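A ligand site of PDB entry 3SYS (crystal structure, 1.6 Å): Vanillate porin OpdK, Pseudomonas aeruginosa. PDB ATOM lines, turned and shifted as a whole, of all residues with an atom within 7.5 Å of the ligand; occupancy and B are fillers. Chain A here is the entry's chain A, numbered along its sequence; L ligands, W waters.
N of Ala 60 lies close to O1 of the ligand (3.5 Å). An oxygen (O4) of the ligand sits at hydrogen-bond distance from the backbone carbonyl oxygen of Ala 60, 2.7 Å away. An oxygen (O2) of the ligand is in hydrogen-bond range of the backbone NH (N) of Leu 114 (2.9 Å). An oxygen (O4) of the ligand sits at hydrogen-bond distance from the backbone NH (N) of Phe 45, 3.4 Å away. The backbone carbonyl oxygen (O) of Phe 45 is in hydrogen-bond range of an oxygen (O4) of the ligand, 3.3 Å away.
The backbone carbonyl oxygen of Phe 45 is in hydrogen-bond range of the backbone NH of Ala 60, at 2.8 Å. N of Glu 112 is in hydrogen-bond range of O of Val 97. OG1 of Thr 131 lies within hydrogen-bond range of OE2 of Glu 112, 2.7 Å away. The backbone carbonyl oxygen of Asp 12 is in hydrogen-bond range of the backbone NH of Lys 44 (2.7 Å). The backbone carbonyl oxygen of Gly 96 is in hydrogen-bond range of the backbone NH of Ile 61 (2.8 Å). O of Asp 59 sits at hydrogen-bond distance from N of Ala 98 (2.8 Å). The side-chain carboxylate (OD1) of Asp 59 sits at hydrogen-bond distance from the side-chain hydroxyl (OG) of Ser 46. NZ of Lys 100 is in salt-bridge range of OD1 of Asp 59 (2.7 Å).
Merely in contact with the ligand: Glu 112, Met 113, Lys 44, Ile 61 and Asp 59. The nearest printed residue that does not touch the ligand is Gly 96 (4.2 Å).
Water W4 lies within hydrogen-bond range of the backbone carbonyl oxygen of Leu 114 (2.6 Å) and an oxygen (O3) of the ligand (2.8 Å). Water W3 bridges NZ of Lys 109 and O2 of the ligand. Water W2 lies within hydrogen-bond range of NZ of Lys 44 (2.8 Å) and O3 of the ligand (3.0 Å). Water W1 lies within hydrogen-bond range of the side-chain carboxylate (OD2) of Asp 59, the side-chain amino group (NZ) of Lys 109 and an oxygen (O2) of the ligand.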
ATOM      1  N   LYS A  10     -25.534 -40.938 -20.764  1.00  0.00           N
ATOM      2  CA  LYS A  10     -25.631 -40.839 -22.214  1.00  0.00           C
ATOM      3  C   LYS A  10     -24.702 -39.760 -22.755  1.00  0.00           C
ATOM      4  O   LYS A  10     -24.503 -38.728 -22.117  1.00  0.00           O
ATOM      5  CB  LYS A  10     -27.079 -40.584 -22.647  1.00  0.00           C
ATOM      6  CG  LYS A  10     -27.744 -39.399 -21.953  1.00  0.00           C
ATOM      7  CD  LYS A  10     -29.223 -39.330 -22.291  1.00  0.00           C
ATOM      8  CE  LYS A  10     -29.951 -40.608 -21.895  1.00  0.00           C
ATOM      9  NZ  LYS A  10     -31.406 -40.561 -22.236  1.00  0.00           N
ATOM     10  N   ASP A  12     -23.988 -37.423 -26.196  1.00  0.00           N
ATOM     11  CA  ASP A  12     -24.500 -36.975 -27.494  1.00  0.00           C
ATOM     12  C   ASP A  12     -23.536 -35.985 -28.118  1.00  0.00           C
ATOM     13  O   ASP A  12     -23.136 -35.009 -27.494  1.00  0.00           O
ATOM     14  CB  ASP A  12     -25.875 -36.327 -27.332  1.00  0.00           C
ATOM     15  CG  ASP A  12     -26.970 -37.343 -27.030  1.00  0.00           C
ATOM     16  OD1 ASP A  12     -27.482 -37.959 -27.981  1.00  0.00           O
ATOM     17  OD2 ASP A  12     -27.309 -37.504 -25.838  1.00  0.00           O
ATOM     18  N   LEU A  43     -20.931 -31.196 -27.715  1.00  0.00           N
ATOM     19  CA  LEU A  43     -20.809 -32.458 -27.024  1.00  0.00           C
ATOM     20  C   LEU A  43     -21.523 -32.368 -25.700  1.00  0.00           C
ATOM     21  O   LEU A  43     -21.223 -31.506 -24.879  1.00  0.00           O
ATOM     22  CB  LEU A  43     -19.326 -32.771 -26.822  1.00  0.00           C
ATOM     23  CG  LEU A  43     -18.975 -34.049 -26.045  1.00  0.00           C
ATOM     24  CD1 LEU A  43     -19.490 -35.288 -26.748  1.00  0.00           C
ATOM     25  CD2 LEU A  43     -17.466 -34.122 -25.856  1.00  0.00           C
ATOM     26  N   LYS A  44     -22.507 -33.244 -25.495  1.00  0.00           N
ATOM     27  CA  LYS A  44     -23.249 -33.257 -24.241  1.00  0.00           C
ATOM     28  C   LYS A  44     -23.062 -34.588 -23.521  1.00  0.00           C
ATOM     29  O   LYS A  44     -23.358 -35.647 -24.066  1.00  0.00           O
ATOM     30  CB  LYS A  44     -24.746 -33.030 -24.493  1.00  0.00           C
ATOM     31  CG  LYS A  44     -25.098 -31.612 -24.934  1.00  0.00           C
ATOM     32  CD  LYS A  44     -26.580 -31.525 -25.326  1.00  0.00           C
ATOM     33  CE  LYS A  44     -26.989 -30.105 -25.653  1.00  0.00           C
ATOM     34  NZ  LYS A  44     -28.421 -30.021 -26.078  1.00  0.00           N
ATOM     35  N   PHE A  45     -22.564 -34.521 -22.283  1.00  0.00           N
ATOM     36  CA  PHE A  45     -22.395 -35.703 -21.445  1.00  0.00           C
ATOM     37  C   PHE A  45     -23.373 -35.588 -20.286  1.00  0.00           C
ATOM     38  O   PHE A  45     -23.265 -34.665 -19.481  1.00  0.00           O
ATOM     39  CB  PHE A  45     -20.989 -35.773 -20.862  1.00  0.00           C
ATOM     40  CG  PHE A  45     -19.906 -36.007 -21.865  1.00  0.00           C
ATOM     41  N   SER A  46     -24.320 -36.512 -20.191  1.00  0.00           N
ATOM     42  CA  SER A  46     -25.317 -36.463 -19.127  1.00  0.00           C
ATOM     43  C   SER A  46     -25.308 -37.766 -18.344  1.00  0.00           C
ATOM     44  O   SER A  46     -25.637 -38.820 -18.885  1.00  0.00           O
ATOM     45  CB  SER A  46     -26.703 -36.216 -19.713  1.00  0.00           C
ATOM     46  OG  SER A  46     -27.666 -36.054 -18.692  1.00  0.00           O
ATOM     47  N   SER A  47     -24.937 -37.695 -17.075  1.00  0.00           N
ATOM     48  CA  SER A  47     -24.826 -38.897 -16.262  1.00  0.00           C
ATOM     49  C   SER A  47     -26.200 -39.387 -15.845  1.00  0.00           C
ATOM     50  O   SER A  47     -27.197 -38.693 -16.024  1.00  0.00           O
ATOM     51  CB  SER A  47     -23.985 -38.639 -15.014  1.00  0.00           C
ATOM     52  OG  SER A  47     -24.751 -37.914 -14.071  1.00  0.00           O
ATOM     53  N   LEU A  58     -24.086 -35.520 -12.827  1.00  0.00           N
ATOM     54  CA  LEU A  58     -23.264 -34.474 -13.399  1.00  0.00           C
ATOM     55  C   LEU A  58     -23.543 -34.408 -14.891  1.00  0.00           C
ATOM     56  O   LEU A  58     -23.555 -35.438 -15.573  1.00  0.00           O
ATOM     57  CB  LEU A  58     -21.784 -34.805 -13.165  1.00  0.00           C
ATOM     58  CG  LEU A  58     -20.782 -33.654 -13.277  1.00  0.00           C
ATOM     59  CD1 LEU A  58     -21.038 -32.633 -12.172  1.00  0.00           C
ATOM     60  CD2 LEU A  58     -19.354 -34.204 -13.180  1.00  0.00           C
ATOM     61  N   ASP A  59     -23.770 -33.193 -15.385  1.00  0.00           N
ATOM     62  CA  ASP A  59     -23.876 -32.958 -16.836  1.00  0.00           C
ATOM     63  C   ASP A  59     -22.698 -32.099 -17.266  1.00  0.00           C
ATOM     64  O   ASP A  59     -22.261 -31.216 -16.530  1.00  0.00           O
ATOM     65  CB  ASP A  59     -25.167 -32.205 -17.179  1.00  0.00           C
ATOM     66  CG  ASP A  59     -26.415 -33.047 -17.017  1.00  0.00           C
ATOM     67  OD1 ASP A  59     -26.305 -34.290 -16.914  1.00  0.00           O
ATOM     68  OD2 ASP A  59     -27.507 -32.458 -17.000  1.00  0.00           O
ATOM     69  N   ALA A  60     -22.203 -32.314 -18.480  1.00  0.00           N
ATOM     70  CA  ALA A  60     -21.171 -31.454 -19.003  1.00  0.00           C
ATOM     71  C   ALA A  60     -21.487 -31.137 -20.446  1.00  0.00           C
ATOM     72  O   ALA A  60     -22.142 -31.909 -21.129  1.00  0.00           O
ATOM     73  CB  ALA A  60     -19.803 -32.107 -18.879  1.00  0.00           C
ATOM     74  N   ILE A  61     -21.037 -29.974 -20.906  1.00  0.00           N
ATOM     75  CA  ILE A  61     -21.219 -29.602 -22.297  1.00  0.00           C
ATOM     76  C   ILE A  61     -19.926 -29.021 -22.832  1.00  0.00           C
ATOM     77  O   ILE A  61     -19.269 -28.211 -22.186  1.00  0.00           O
ATOM     78  CB  ILE A  61     -22.403 -28.619 -22.486  1.00  0.00           C
ATOM     79  CG1 ILE A  61     -22.669 -28.362 -23.974  1.00  0.00           C
ATOM     80  CG2 ILE A  61     -22.149 -27.308 -21.760  1.00  0.00           C
ATOM     81  CD1 ILE A  61     -23.934 -27.524 -24.214  1.00  0.00           C
ATOM     82  N   GLY A  62     -19.549 -29.500 -24.012  1.00  0.00           N
ATOM     83  CA  GLY A  62     -18.372 -29.001 -24.684  1.00  0.00           C
ATOM     84  C   GLY A  62     -18.750 -28.407 -26.015  1.00  0.00           C
ATOM     85  O   GLY A  62     -19.437 -29.054 -26.823  1.00  0.00           O
ATOM     86  N   GLY A  96     -18.565 -26.488 -20.047  1.00  0.00           N
ATOM     87  CA  GLY A  96     -19.386 -26.157 -18.888  1.00  0.00           C
ATOM     88  C   GLY A  96     -19.821 -27.427 -18.185  1.00  0.00           C
ATOM     89  O   GLY A  96     -20.010 -28.464 -18.831  1.00  0.00           O
ATOM     90  N   VAL A  97     -19.985 -27.347 -16.872  1.00  0.00           N
ATOM     91  CA  VAL A  97     -20.431 -28.495 -16.087  1.00  0.00           C
ATOM     92  C   VAL A  97     -21.551 -28.064 -15.150  1.00  0.00           C
ATOM     93  O   VAL A  97     -21.580 -26.926 -14.685  1.00  0.00           O
ATOM     94  CB  VAL A  97     -19.267 -29.072 -15.258  1.00  0.00           C
ATOM     95  CG1 VAL A  97     -19.728 -30.279 -14.466  1.00  0.00           C
ATOM     96  CG2 VAL A  97     -18.096 -29.468 -16.162  1.00  0.00           C
ATOM     97  N   ALA A  98     -22.491 -28.965 -14.884  1.00  0.00           N
ATOM     98  CA  ALA A  98     -23.532 -28.718 -13.897  1.00  0.00           C
ATOM     99  C   ALA A  98     -23.697 -29.935 -13.010  1.00  0.00           C
ATOM    100  O   ALA A  98     -23.707 -31.069 -13.492  1.00  0.00           O
ATOM    101  CB  ALA A  98     -24.859 -28.373 -14.572  1.00  0.00           C
ATOM    102  N   ALA A  99     -23.801 -29.719 -11.709  1.00  0.00           N
ATOM    103  CA  ALA A  99     -24.148 -30.813 -10.816  1.00  0.00           C
ATOM    104  C   ALA A  99     -25.665 -30.934 -10.772  1.00  0.00           C
ATOM    105  O   ALA A  99     -26.371 -29.935 -10.884  1.00  0.00           O
ATOM    106  CB  ALA A  99     -23.601 -30.544  -9.408  1.00  0.00           C
ATOM    107  N   LYS A 100     -26.163 -32.147 -10.608  1.00  0.00           N
ATOM    108  CA  LYS A 100     -27.596 -32.328 -10.451  1.00  0.00           C
ATOM    109  C   LYS A 100     -27.920 -33.151  -9.228  1.00  0.00           C
ATOM    110  O   LYS A 100     -27.180 -34.077  -8.867  1.00  0.00           O
ATOM    111  CB  LYS A 100     -28.236 -32.905 -11.713  1.00  0.00           C
ATOM    112  CG  LYS A 100     -27.619 -34.176 -12.247  1.00  0.00           C
ATOM    113  CD  LYS A 100     -28.078 -34.410 -13.689  1.00  0.00           C
ATOM    114  CE  LYS A 100     -27.543 -35.721 -14.228  1.00  0.00           C
ATOM    115  NZ  LYS A 100     -28.002 -35.942 -15.641  1.00  0.00           N
ATOM    116  N   LYS A 109     -30.388 -28.248 -10.314  1.00  0.00           N
ATOM    117  CA  LYS A 109     -29.158 -28.232 -11.099  1.00  0.00           C
ATOM    118  C   LYS A 109     -28.353 -26.967 -10.776  1.00  0.00           C
ATOM    119  O   LYS A 109     -28.934 -25.879 -10.628  1.00  0.00           O
ATOM    120  CB  LYS A 109     -29.452 -28.314 -12.601  1.00  0.00           C
ATOM    121  CG  LYS A 109     -30.106 -29.630 -13.006  1.00  0.00           C
ATOM    122  CD  LYS A 109     -29.534 -30.161 -14.323  1.00  0.00           C
ATOM    123  CE  LYS A 109     -30.483 -29.949 -15.485  1.00  0.00           C
ATOM    124  NZ  LYS A 109     -30.691 -28.516 -15.795  1.00  0.00           N
ATOM    125  N   GLY A 111     -24.756 -24.874 -11.912  1.00  0.00           N
ATOM    126  CA  GLY A 111     -23.613 -24.773 -12.794  1.00  0.00           C
ATOM    127  C   GLY A 111     -24.016 -24.191 -14.137  1.00  0.00           C
ATOM    128  O   GLY A 111     -24.803 -23.250 -14.191  1.00  0.00           O
ATOM    129  N   GLU A 112     -23.474 -24.755 -15.219  1.00  0.00           N
ATOM    130  CA  GLU A 112     -23.745 -24.218 -16.546  1.00  0.00           C
ATOM    131  C   GLU A 112     -24.820 -25.068 -17.227  1.00  0.00           C
ATOM    132  O   GLU A 112     -24.740 -26.295 -17.212  1.00  0.00           O
ATOM    133  CB  GLU A 112     -22.455 -24.188 -17.375  1.00  0.00           C
ATOM    134  CG  GLU A 112     -22.602 -23.466 -18.713  1.00  0.00           C
ATOM    135  CD  GLU A 112     -21.281 -23.042 -19.271  1.00  0.00           C
ATOM    136  OE1 GLU A 112     -20.310 -22.969 -18.487  1.00  0.00           O
ATOM    137  OE2 GLU A 112     -21.211 -22.798 -20.493  1.00  0.00           O
ATOM    138  N   MET A 113     -25.826 -24.405 -17.791  1.00  0.00           N
ATOM    139  CA  MET A 113     -26.952 -25.114 -18.367  1.00  0.00           C
ATOM    140  C   MET A 113     -27.635 -24.289 -19.471  1.00  0.00           C
ATOM    141  O   MET A 113     -27.194 -23.185 -19.790  1.00  0.00           O
ATOM    142  CB  MET A 113     -27.955 -25.520 -17.286  1.00  0.00           C
ATOM    143  CG  MET A 113     -28.555 -24.379 -16.515  1.00  0.00           C
ATOM    144  SD  MET A 113     -29.229 -24.927 -14.914  1.00  0.00           S
ATOM    145  CE  MET A 113     -27.733 -25.001 -13.930  1.00  0.00           C
ATOM    146  N   LEU A 114     -28.684 -24.867 -20.046  1.00  0.00           N
ATOM    147  CA  LEU A 114     -29.377 -24.306 -21.203  1.00  0.00           C
ATOM    148  C   LEU A 114     -30.844 -24.078 -20.807  1.00  0.00           C
ATOM    149  O   LEU A 114     -31.713 -24.908 -21.113  1.00  0.00           O
ATOM    150  CB  LEU A 114     -29.314 -25.313 -22.358  1.00  0.00           C
ATOM    151  CG  LEU A 114     -27.914 -25.675 -22.866  1.00  0.00           C
ATOM    152  CD1 LEU A 114     -27.975 -26.970 -23.689  1.00  0.00           C
ATOM    153  CD2 LEU A 114     -27.359 -24.557 -23.703  1.00  0.00           C
ATOM    154  N   PRO A 115     -31.119 -22.986 -20.104  1.00  0.00           N
ATOM    155  CA  PRO A 115     -32.514 -22.775 -19.664  1.00  0.00           C
ATOM    156  C   PRO A 115     -33.458 -22.610 -20.838  1.00  0.00           C
ATOM    157  O   PRO A 115     -33.165 -21.881 -21.785  1.00  0.00           O
ATOM    158  CB  PRO A 115     -32.443 -21.486 -18.849  1.00  0.00           C
ATOM    159  CG  PRO A 115     -31.155 -20.804 -19.257  1.00  0.00           C
ATOM    160  CD  PRO A 115     -30.215 -21.890 -19.700  1.00  0.00           C
ATOM    161  N   ASP A 116     -34.609 -23.260 -20.752  1.00  0.00           N
ATOM    162  CA  ASP A 116     -35.603 -23.182 -21.808  1.00  0.00           C
ATOM    163  C   ASP A 116     -36.959 -22.979 -21.146  1.00  0.00           C
ATOM    164  O   ASP A 116     -37.787 -23.892 -21.076  1.00  0.00           O
ATOM    165  CB  ASP A 116     -35.578 -24.461 -22.641  1.00  0.00           C
ATOM    166  CG  ASP A 116     -36.387 -24.342 -23.921  1.00  0.00           C
ATOM    167  OD1 ASP A 116     -36.726 -23.223 -24.335  1.00  0.00           O
ATOM    168  OD2 ASP A 116     -36.651 -25.409 -24.532  1.00  0.00           O
ATOM    169  N   TYR A 122     -32.959 -20.063 -24.097  1.00  0.00           N
ATOM    170  CA  TYR A 122     -31.588 -20.051 -24.605  1.00  0.00           C
ATOM    171  C   TYR A 122     -31.590 -20.055 -26.138  1.00  0.00           C
ATOM    172  O   TYR A 122     -32.392 -20.737 -26.784  1.00  0.00           O
ATOM    173  CB  TYR A 122     -30.758 -21.219 -24.051  1.00  0.00           C
ATOM    174  CG  TYR A 122     -30.938 -22.548 -24.743  1.00  0.00           C
ATOM    175  CD1 TYR A 122     -30.020 -22.970 -25.700  1.00  0.00           C
ATOM    176  CD2 TYR A 122     -32.002 -23.380 -24.433  1.00  0.00           C
ATOM    177  CE1 TYR A 122     -30.170 -24.198 -26.332  1.00  0.00           C
ATOM    178  CE2 TYR A 122     -32.153 -24.609 -25.065  1.00  0.00           C
ATOM    179  CZ  TYR A 122     -31.239 -25.004 -26.006  1.00  0.00           C
ATOM    180  OH  TYR A 122     -31.381 -26.214 -26.639  1.00  0.00           O
ATOM    181  N   THR A 131     -25.296 -20.373 -23.398  1.00  0.00           N
ATOM    182  CA  THR A 131     -25.415 -21.071 -22.113  1.00  0.00           C
ATOM    183  C   THR A 131     -25.433 -20.063 -20.961  1.00  0.00           C
ATOM    184  O   THR A 131     -25.058 -18.906 -21.124  1.00  0.00           O
ATOM    185  CB  THR A 131     -24.282 -22.071 -21.878  1.00  0.00           C
ATOM    186  OG1 THR A 131     -23.018 -21.389 -21.911  1.00  0.00           O
ATOM    187  CG2 THR A 131     -24.296 -23.176 -22.917  1.00  0.00           C
HETATM  188  C1  LIG L   1     -27.946 -29.622 -20.634  1.00  0.00           C
HETATM  189  C2  LIG L   1     -28.149 -30.829 -21.286  1.00  0.00           C
HETATM  190  C3  LIG L   1     -26.693 -29.325 -20.119  1.00  0.00           C
HETATM  191  C4  LIG L   1     -27.096 -31.721 -21.457  1.00  0.00           C
HETATM  192  C5  LIG L   1     -25.632 -30.219 -20.278  1.00  0.00           C
HETATM  193  O1  LIG L   1     -24.374 -29.927 -19.793  1.00  0.00           O
HETATM  194  C6  LIG L   1     -25.846 -31.412 -20.955  1.00  0.00           C
HETATM  195  C7  LIG L   1     -29.110 -28.704 -20.462  1.00  0.00           C
HETATM  196  C8  LIG L   1     -24.198 -28.893 -18.883  1.00  0.00           C
HETATM  197  O2  LIG L   1     -29.075 -27.758 -19.631  1.00  0.00           O
HETATM  198  O3  LIG L   1     -30.152 -28.922 -21.142  1.00  0.00           O
HETATM  199  O4  LIG L   1     -24.809 -32.285 -21.111  1.00  0.00           O
HETATM  200  O   HOH W   1     -27.987 -29.761 -17.226  1.00  0.00           O
HETATM  201  O   HOH W   2     -30.277 -29.940 -23.958  1.00  0.00           O
HETATM  202  O   HOH W   3     -31.427 -27.034 -18.131  1.00  0.00           O
HETATM  203  O   HOH W   4     -32.270 -27.276 -22.028  1.00  0.00           O
